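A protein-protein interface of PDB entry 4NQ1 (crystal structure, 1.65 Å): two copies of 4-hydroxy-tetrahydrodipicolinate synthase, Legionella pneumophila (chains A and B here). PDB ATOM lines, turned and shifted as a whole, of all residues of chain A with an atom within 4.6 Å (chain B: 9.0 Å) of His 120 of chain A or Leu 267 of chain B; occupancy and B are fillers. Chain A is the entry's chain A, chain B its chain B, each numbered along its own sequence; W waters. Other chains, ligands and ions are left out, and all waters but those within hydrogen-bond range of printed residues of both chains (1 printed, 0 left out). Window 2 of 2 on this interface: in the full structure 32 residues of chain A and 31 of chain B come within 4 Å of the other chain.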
ATOM      1  N   ASN A  79     -21.646 -14.672  21.724  1.00  0.00           N
ATOM      2  CA  ASN A  79     -22.893 -15.073  21.070  1.00  0.00           C
ATOM      3  C   ASN A  79     -22.906 -14.972  19.591  1.00  0.00           C
ATOM      4  O   ASN A  79     -23.248 -15.947  18.941  1.00  0.00           O
ATOM      5  CB  ASN A  79     -24.068 -14.212  21.600  1.00  0.00           C
ATOM      6  CG  ASN A  79     -24.630 -14.764  22.899  1.00  0.00           C
ATOM      7  OD1 ASN A  79     -24.172 -15.778  23.427  1.00  0.00           O
ATOM      8  ND2 ASN A  79     -25.620 -14.076  23.434  1.00  0.00           N
ATOM      9  N   ALA A  80     -22.483 -13.831  19.040  1.00  0.00           N
ATOM     10  CA  ALA A  80     -22.415 -13.681  17.569  1.00  0.00           C
ATOM     11  C   ALA A  80     -21.225 -14.463  17.041  1.00  0.00           C
ATOM     12  O   ALA A  80     -20.113 -14.306  17.541  1.00  0.00           O
ATOM     13  CB  ALA A  80     -22.250 -12.202  17.199  1.00  0.00           C
ATOM     14  N   THR A  81     -21.475 -15.234  15.984  1.00  0.00           N
ATOM     15  CA  THR A  81     -20.369 -16.043  15.363  1.00  0.00           C
ATOM     16  C   THR A  81     -19.191 -15.174  14.977  1.00  0.00           C
ATOM     17  O   THR A  81     -18.045 -15.522  15.245  1.00  0.00           O
ATOM     18  CB  THR A  81     -20.945 -16.766  14.135  1.00  0.00           C
ATOM     19  OG1 THR A  81     -22.108 -17.483  14.530  1.00  0.00           O
ATOM     20  CG2 THR A  81     -19.924 -17.815  13.642  1.00  0.00           C
ATOM     21  N   ILE A  85     -15.406 -15.551  16.429  1.00  0.00           N
ATOM     22  CA  ILE A  85     -14.219 -15.765  15.576  1.00  0.00           C
ATOM     23  C   ILE A  85     -13.090 -14.767  15.975  1.00  0.00           C
ATOM     24  O   ILE A  85     -11.933 -15.179  16.079  1.00  0.00           O
ATOM     25  CB  ILE A  85     -14.607 -15.539  14.123  1.00  0.00           C
ATOM     26  CG1 ILE A  85     -15.328 -16.789  13.557  1.00  0.00           C
ATOM     27  CG2 ILE A  85     -13.311 -15.211  13.175  1.00  0.00           C
ATOM     28  CD1 ILE A  85     -16.097 -16.546  12.249  1.00  0.00           C
ATOM     29  N   LEU A 116     -23.453 -24.343  12.243  1.00  0.00           N
ATOM     30  CA  LEU A 116     -22.887 -23.238  11.447  1.00  0.00           C
ATOM     31  C   LEU A 116     -21.917 -22.406  12.307  1.00  0.00           C
ATOM     32  O   LEU A 116     -20.826 -21.965  11.802  1.00  0.00           O
ATOM     33  CB  LEU A 116     -23.976 -22.337  10.836  1.00  0.00           C
ATOM     34  CG  LEU A 116     -24.761 -23.152   9.790  1.00  0.00           C
ATOM     35  CD1 LEU A 116     -25.956 -22.258   9.463  1.00  0.00           C
ATOM     36  CD2 LEU A 116     -23.912 -23.442   8.507  1.00  0.00           C
ATOM     37  N   HIS A 117     -22.320 -22.143  13.561  1.00  0.00           N
ATOM     38  CA  HIS A 117     -21.476 -21.319  14.462  1.00  0.00           C
ATOM     39  C   HIS A 117     -20.058 -21.929  14.588  1.00  0.00           C
ATOM     40  O   HIS A 117     -19.020 -21.311  14.319  1.00  0.00           O
ATOM     41  CB  HIS A 117     -22.199 -21.279  15.854  1.00  0.00           C
ATOM     42  CG  HIS A 117     -21.551 -20.422  16.877  1.00  0.00           C
ATOM     43  ND1 HIS A 117     -21.581 -19.022  16.853  1.00  0.00           N
ATOM     44  CD2 HIS A 117     -21.010 -20.770  18.057  1.00  0.00           C
ATOM     45  CE1 HIS A 117     -21.079 -18.572  17.989  1.00  0.00           C
ATOM     46  NE2 HIS A 117     -20.710 -19.607  18.719  1.00  0.00           N
ATOM     47  N   TYR A 118     -20.033 -23.173  15.031  1.00  0.00           N
ATOM     48  CA  TYR A 118     -18.737 -23.836  15.314  1.00  0.00           C
ATOM     49  C   TYR A 118     -17.983 -24.153  14.034  1.00  0.00           C
ATOM     50  O   TYR A 118     -16.751 -24.087  14.002  1.00  0.00           O
ATOM     51  CB  TYR A 118     -18.995 -25.114  16.107  1.00  0.00           C
ATOM     52  CG  TYR A 118     -19.347 -24.846  17.572  1.00  0.00           C
ATOM     53  CD1 TYR A 118     -18.371 -24.292  18.450  1.00  0.00           C
ATOM     54  CD2 TYR A 118     -20.640 -25.043  18.038  1.00  0.00           C
ATOM     55  CE1 TYR A 118     -18.680 -24.022  19.794  1.00  0.00           C
ATOM     56  CE2 TYR A 118     -20.973 -24.789  19.371  1.00  0.00           C
ATOM     57  CZ  TYR A 118     -19.982 -24.303  20.237  1.00  0.00           C
ATOM     58  OH  TYR A 118     -20.261 -24.123  21.554  1.00  0.00           O
ATOM     59  N   SER A 119     -18.680 -24.524  12.963  1.00  0.00           N
ATOM     60  CA  SER A 119     -17.944 -24.813  11.712  1.00  0.00           C
ATOM     61  C   SER A 119     -17.340 -23.516  11.105  1.00  0.00           C
ATOM     62  O   SER A 119     -16.218 -23.519  10.557  1.00  0.00           O
ATOM     63  CB  SER A 119     -18.863 -25.569  10.714  1.00  0.00           C
ATOM     64  OG  SER A 119     -19.940 -24.745  10.331  1.00  0.00           O
ATOM     65  N   HIS A 120     -18.058 -22.383  11.214  1.00  0.00           N
ATOM     66  CA  HIS A 120     -17.455 -21.097  10.798  1.00  0.00           C
ATOM     67  C   HIS A 120     -16.259 -20.734  11.646  1.00  0.00           C
ATOM     68  O   HIS A 120     -15.232 -20.293  11.106  1.00  0.00           O
ATOM     69  CB  HIS A 120     -18.515 -19.951  10.857  1.00  0.00           C
ATOM     70  CG  HIS A 120     -19.336 -19.831   9.623  1.00  0.00           C
ATOM     71  ND1 HIS A 120     -18.934 -19.045   8.559  1.00  0.00           N
ATOM     72  CD2 HIS A 120     -20.557 -20.325   9.291  1.00  0.00           C
ATOM     73  CE1 HIS A 120     -19.869 -19.075   7.619  1.00  0.00           C
ATOM     74  NE2 HIS A 120     -20.852 -19.860   8.027  1.00  0.00           N
ATOM     75  N   ILE A 121     -16.374 -20.866  12.988  1.00  0.00           N
ATOM     76  CA  ILE A 121     -15.242 -20.528  13.839  1.00  0.00           C
ATOM     77  C   ILE A 121     -14.020 -21.414  13.475  1.00  0.00           C
ATOM     78  O   ILE A 121     -12.894 -20.903  13.312  1.00  0.00           O
ATOM     79  CB  ILE A 121     -15.588 -20.728  15.317  1.00  0.00           C
ATOM     80  CG1 ILE A 121     -16.706 -19.728  15.708  1.00  0.00           C
ATOM     81  CG2 ILE A 121     -14.367 -20.421  16.211  1.00  0.00           C
ATOM     82  CD1 ILE A 121     -17.489 -20.126  17.004  1.00  0.00           C
ATOM     83  N   ALA A 122     -14.248 -22.744  13.390  1.00  0.00           N
ATOM     84  CA  ALA A 122     -13.129 -23.681  13.097  1.00  0.00           C
ATOM     85  C   ALA A 122     -12.532 -23.400  11.712  1.00  0.00           C
ATOM     86  O   ALA A 122     -11.325 -23.501  11.563  1.00  0.00           O
ATOM     87  CB  ALA A 122     -13.654 -25.152  13.155  1.00  0.00           C
ATOM     88  N   GLN A 123     -13.327 -23.033  10.693  1.00  0.00           N
ATOM     89  CA  GLN A 123     -12.749 -22.730   9.362  1.00  0.00           C
ATOM     90  C   GLN A 123     -11.927 -21.443   9.332  1.00  0.00           C
ATOM     91  O   GLN A 123     -11.008 -21.293   8.527  1.00  0.00           O
ATOM     92  CB  GLN A 123     -13.916 -22.514   8.399  1.00  0.00           C
ATOM     93  CG  GLN A 123     -14.552 -23.720   8.016  1.00  0.00           C
ATOM     94  CD  GLN A 123     -15.719 -23.419   7.035  1.00  0.00           C
ATOM     95  OE1 GLN A 123     -15.482 -23.070   5.842  1.00  0.00           O
ATOM     96  NE2 GLN A 123     -16.967 -23.572   7.508  1.00  0.00           N
ATOM     97  N   SER A 124     -12.279 -20.518  10.223  1.00  0.00           N
ATOM     98  CA  SER A 124     -11.693 -19.186  10.273  1.00  0.00           C
ATOM     99  C   SER A 124     -10.467 -19.123  11.153  1.00  0.00           C
ATOM    100  O   SER A 124      -9.592 -18.290  10.882  1.00  0.00           O
ATOM    101  CB  SER A 124     -12.705 -18.188  10.841  1.00  0.00           C
ATOM    102  OG  SER A 124     -13.776 -18.092   9.927  1.00  0.00           O
ATOM    103  N   MET B  13     -31.980  -6.078   9.119  1.00  0.00           N
ATOM    104  CA  MET B  13     -30.556  -6.259   8.813  1.00  0.00           C
ATOM    105  C   MET B  13     -30.355  -6.313   7.302  1.00  0.00           C
ATOM    106  O   MET B  13     -31.217  -6.798   6.604  1.00  0.00           O
ATOM    107  CB  MET B  13     -30.064  -7.595   9.443  1.00  0.00           C
ATOM    108  CG  MET B  13     -29.767  -7.432  10.912  1.00  0.00           C
ATOM    109  SD  MET B  13     -29.573  -9.030  11.724  1.00  0.00           S
ATOM    110  CE  MET B  13     -29.271  -8.519  13.446  1.00  0.00           C
ATOM    111  N   ASP B  16     -25.363  -7.799   6.917  1.00  0.00           N
ATOM    112  CA  ASP B  16     -24.904  -7.939   8.316  1.00  0.00           C
ATOM    113  C   ASP B  16     -24.723  -6.612   9.060  1.00  0.00           C
ATOM    114  O   ASP B  16     -23.930  -6.530   9.954  1.00  0.00           O
ATOM    115  CB  ASP B  16     -23.671  -8.880   8.444  1.00  0.00           C
ATOM    116  CG  ASP B  16     -23.515  -9.449   9.874  1.00  0.00           C
ATOM    117  OD1 ASP B  16     -24.580  -9.722  10.484  1.00  0.00           O
ATOM    118  OD2 ASP B  16     -22.350  -9.579  10.280  1.00  0.00           O
ATOM    119  N   GLU B  46     -32.786  -9.018  18.349  1.00  0.00           N
ATOM    120  CA  GLU B  46     -31.459  -9.641  18.292  1.00  0.00           C
ATOM    121  C   GLU B  46     -30.415  -8.952  19.182  1.00  0.00           C
ATOM    122  O   GLU B  46     -29.215  -8.910  18.875  1.00  0.00           O
ATOM    123  CB  GLU B  46     -30.982  -9.869  16.808  1.00  0.00           C
ATOM    124  CG  GLU B  46     -31.740 -11.052  16.132  1.00  0.00           C
ATOM    125  CD  GLU B  46     -31.513 -11.045  14.618  1.00  0.00           C
ATOM    126  OE1 GLU B  46     -32.355 -10.396  13.899  1.00  0.00           O
ATOM    127  OE2 GLU B  46     -30.440 -11.619  14.204  1.00  0.00           O
ATOM    128  N   GLY B  48     -29.044 -10.021  21.619  1.00  0.00           N
ATOM    129  CA  GLY B  48     -28.020 -10.981  22.017  1.00  0.00           C
ATOM    130  C   GLY B  48     -26.826 -11.054  21.052  1.00  0.00           C
ATOM    131  O   GLY B  48     -25.802 -11.602  21.406  1.00  0.00           O
ATOM    132  N   THR B  49     -27.012 -10.580  19.814  1.00  0.00           N
ATOM    133  CA  THR B  49     -25.855 -10.648  18.854  1.00  0.00           C
ATOM    134  C   THR B  49     -25.499  -9.262  18.301  1.00  0.00           C
ATOM    135  O   THR B  49     -24.514  -9.135  17.504  1.00  0.00           O
ATOM    136  CB  THR B  49     -26.127 -11.568  17.628  1.00  0.00           C
ATOM    137  OG1 THR B  49     -27.282 -11.057  16.949  1.00  0.00           O
ATOM    138  CG2 THR B  49     -26.295 -13.053  18.030  1.00  0.00           C
ATOM    139  N   LEU B  50     -26.185  -8.218  18.771  1.00  0.00           N
ATOM    140  CA  LEU B  50     -25.797  -6.859  18.362  1.00  0.00           C
ATOM    141  C   LEU B  50     -24.592  -6.329  19.137  1.00  0.00           C
ATOM    142  O   LEU B  50     -24.414  -6.632  20.344  1.00  0.00           O
ATOM    143  CB  LEU B  50     -27.028  -5.940  18.603  1.00  0.00           C
ATOM    144  CG  LEU B  50     -28.276  -6.067  17.696  1.00  0.00           C
ATOM    145  CD1 LEU B  50     -29.276  -4.972  18.091  1.00  0.00           C
ATOM    146  CD2 LEU B  50     -27.866  -5.961  16.195  1.00  0.00           C
ATOM    147  N   GLU B 264     -33.125 -11.131   7.124  1.00  0.00           N
ATOM    148  CA  GLU B 264     -31.821 -11.708   7.428  1.00  0.00           C
ATOM    149  C   GLU B 264     -31.589 -11.770   8.950  1.00  0.00           C
ATOM    150  O   GLU B 264     -31.852 -10.784   9.627  1.00  0.00           O
ATOM    151  CB  GLU B 264     -30.733 -10.870   6.767  1.00  0.00           C
ATOM    152  CG  GLU B 264     -30.948 -10.966   5.258  1.00  0.00           C
ATOM    153  CD  GLU B 264     -29.926 -10.101   4.483  1.00  0.00           C
ATOM    154  OE1 GLU B 264     -28.785 -10.002   4.985  1.00  0.00           O
ATOM    155  OE2 GLU B 264     -30.309  -9.537   3.387  1.00  0.00           O
ATOM    156  N   LEU B 265     -30.989 -12.890   9.392  1.00  0.00           N
ATOM    157  CA  LEU B 265     -30.634 -13.068  10.810  1.00  0.00           C
ATOM    158  C   LEU B 265     -29.135 -13.217  10.935  1.00  0.00           C
ATOM    159  O   LEU B 265     -28.475 -13.801  10.013  1.00  0.00           O
ATOM    160  CB  LEU B 265     -31.258 -14.320  11.283  1.00  0.00           C
ATOM    161  CG  LEU B 265     -32.773 -14.037  11.437  1.00  0.00           C
ATOM    162  CD1 LEU B 265     -33.645 -14.879  10.542  1.00  0.00           C
ATOM    163  CD2 LEU B 265     -33.160 -14.111  12.866  1.00  0.00           C
ATOM    164  N   ARG B 266     -28.592 -12.645  12.006  1.00  0.00           N
ATOM    165  CA  ARG B 266     -27.178 -12.794  12.247  1.00  0.00           C
ATOM    166  C   ARG B 266     -26.867 -14.164  12.852  1.00  0.00           C
ATOM    167  O   ARG B 266     -27.482 -14.543  13.902  1.00  0.00           O
ATOM    168  CB  ARG B 266     -26.704 -11.637  13.112  1.00  0.00           C
ATOM    169  CG  ARG B 266     -25.212 -11.784  13.494  1.00  0.00           C
ATOM    170  CD  ARG B 266     -24.682 -10.533  14.213  1.00  0.00           C
ATOM    171  NE  ARG B 266     -24.580  -9.421  13.277  1.00  0.00           N
ATOM    172  CZ  ARG B 266     -24.442  -8.156  13.659  1.00  0.00           C
ATOM    173  NH1 ARG B 266     -24.410  -7.832  14.958  1.00  0.00           N
ATOM    174  NH2 ARG B 266     -24.357  -7.199  12.731  1.00  0.00           N
ATOM    175  N   LEU B 267     -25.849 -14.837  12.313  1.00  0.00           N
ATOM    176  CA  LEU B 267     -25.418 -16.139  12.861  1.00  0.00           C
ATOM    177  C   LEU B 267     -24.996 -15.936  14.336  1.00  0.00           C
ATOM    178  O   LEU B 267     -24.331 -14.952  14.639  1.00  0.00           O
ATOM    179  CB  LEU B 267     -24.227 -16.747  12.072  1.00  0.00           C
ATOM    180  CG  LEU B 267     -24.676 -17.373  10.731  1.00  0.00           C
ATOM    181  CD1 LEU B 267     -23.419 -17.802   9.972  1.00  0.00           C
ATOM    182  CD2 LEU B 267     -25.557 -18.602  11.079  1.00  0.00           C
ATOM    183  N   PRO B 268     -25.377 -16.852  15.213  1.00  0.00           N
ATOM    184  CA  PRO B 268     -25.808 -18.247  14.935  1.00  0.00           C
ATOM    185  C   PRO B 268     -27.318 -18.402  14.735  1.00  0.00           C
ATOM    186  O   PRO B 268     -27.777 -19.536  14.597  1.00  0.00           O
ATOM    187  CB  PRO B 268     -25.380 -19.016  16.233  1.00  0.00           C
ATOM    188  CG  PRO B 268     -25.548 -17.924  17.292  1.00  0.00           C
ATOM    189  CD  PRO B 268     -24.995 -16.671  16.644  1.00  0.00           C
ATOM    190  N   MET B 269     -28.051 -17.286  14.690  1.00  0.00           N
ATOM    191  CA  MET B 269     -29.479 -17.381  14.347  1.00  0.00           C
ATOM    192  C   MET B 269     -29.602 -17.654  12.838  1.00  0.00           C
ATOM    193  O   MET B 269     -28.749 -17.235  12.086  1.00  0.00           O
ATOM    194  CB  MET B 269     -30.294 -16.143  14.792  1.00  0.00           C
ATOM    195  CG  MET B 269     -30.065 -15.836  16.293  1.00  0.00           C
ATOM    196  SD  MET B 269     -30.279 -17.252  17.459  1.00  0.00           S
ATOM    197  CE  MET B 269     -32.057 -17.495  17.286  1.00  0.00           C
ATOM    198  N   THR B 270     -30.619 -18.432  12.471  1.00  0.00           N
ATOM    199  CA  THR B 270     -30.754 -18.985  11.105  1.00  0.00           C
ATOM    200  C   THR B 270     -32.161 -18.676  10.581  1.00  0.00           C
ATOM    201  O   THR B 270     -33.141 -18.574  11.346  1.00  0.00           O
ATOM    202  CB  THR B 270     -30.631 -20.537  11.146  1.00  0.00           C
ATOM    203  OG1 THR B 270     -31.395 -21.094  12.252  1.00  0.00           O
ATOM    204  CG2 THR B 270     -29.092 -20.926  11.348  1.00  0.00           C
ATOM    205  N   GLU B 271     -32.274 -18.444   9.272  1.00  0.00           N
ATOM    206  CA  GLU B 271     -33.637 -18.240   8.706  1.00  0.00           C
ATOM    207  C   GLU B 271     -34.516 -19.499   8.930  1.00  0.00           C
ATOM    208  O   GLU B 271     -33.995 -20.627   8.969  1.00  0.00           O
ATOM    209  CB  GLU B 271     -33.528 -17.818   7.194  1.00  0.00           C
ATOM    210  CG  GLU B 271     -32.765 -16.515   7.037  1.00  0.00           C
ATOM    211  CD  GLU B 271     -32.492 -16.079   5.597  1.00  0.00           C
ATOM    212  OE1 GLU B 271     -33.254 -16.422   4.701  1.00  0.00           O
ATOM    213  OE2 GLU B 271     -31.468 -15.428   5.376  1.00  0.00           O
HETATM  214  O   HOH W   1     -22.245 -13.391  13.517  1.00  0.00           O
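The side-chain amide nitrogen (ND2) of Asn 79 of chain A sits close to the backbone carbonyl oxygen (O) of Gly 48 of chain B (3.2 Å).
O of Leu 267 of chain B sits at hydrogen-bond distance from N of Thr 81 of chain A.
The side-chain hydroxyl (OG1) of Thr 81 of chain A lies close to the backbone nitrogen (N) of Pro 268 of chain B (3.4 Å).
The side-chain hydroxyl (OG1) of Thr 81 of chain A is in hydrogen-bond range of a ring nitrogen (ND1) of His 117 of chain A (2.8 Å).
The backbone carbonyl oxygen (O) of Leu 116 of chain A sits at hydrogen-bond distance from the side-chain hydroxyl (OG) of Ser 119 of chain A (3.3 Å).
The backbone carbonyl oxygen (O) of His 120 of chain A is in hydrogen-bond range of the side-chain hydroxyl (OG) of Ser 124 of chain A (2.9 Å).
The side-chain hydroxyl (OG1) of Thr 49 of chain B lies within hydrogen-bond range of the backbone carbonyl oxygen (O) of Glu 46 of chain B (3.5 Å).
NH1 of Arg 266 of chain B is in hydrogen-bond range of O of Thr 49 of chain B (2.9 Å).
Among the printed residues, merely in contact across the chains: Asn 79 of chain A with Pro 268 of chain B, Ala 80 of chain A with Thr 49 of chain B, Ala 80 of chain A with Leu 267 of chain B, Leu 116 of chain A with Thr 270 of chain B, His 117 of chain A with Pro 268 of chain B and His 120 of chain A with Leu 267 of chain B.
Of the printed residues of chain B, His 120 of chain A touches Leu 267.
Printed residues of chain A within 4 Å of Leu 267 of chain B: Ala 80 (3.7 Å), Thr 81 (3.2 Å) and His 120 (3.8 Å).
Printed residues of chain B within 4 Å of Thr 81 of chain A: Leu 267 and Pro 268.
Printed residues of chain B within 4 Å of Ala 80 of chain A: Thr 49 and Leu 267.
Printed residues of chain A within 4 Å of Gly 48 of chain B: Asn 79 (3.1 Å).
Of the printed residues of chain A, Pro 268 of chain B touches Asn 79 (3.0 Å), Thr 81 (3.4 Å) and His 117 (3.8 Å).
The nearest printed residue of chain A that does not touch Leu 267 of chain B is Leu 116 of chain A (4.02 Å).
The nearest printed residue of chain B that does not touch Thr 81 of chain A is Arg 266 of chain B (5.7 Å).
Of the 13 printed residues of chain A, 6 touch a printed residue of chain B.
Printed residues of chain A that touch a printed residue of chain B: Asn 79, Ala 80, Thr 81, Leu 116, His 117 and His 120.
Hydrophobic or aromatic side chains of chain B within 4 Å of the printed part of chain A: Leu 267 and Pro 268.
Among the printed residues, no Asp or Glu carboxylate lies within 4 Å of a Lys or Arg side-chain nitrogen of the other chain.
No position is printed for both chains.
Of the 9 pairs that touch across the chains among the printed residues, none has its exchanged pair printed and touching as well.
Water W1 lies within hydrogen-bond range of O of Leu 267 of chain B (2.8 Å) and N of Thr 81 of chain A (3.2 Å).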
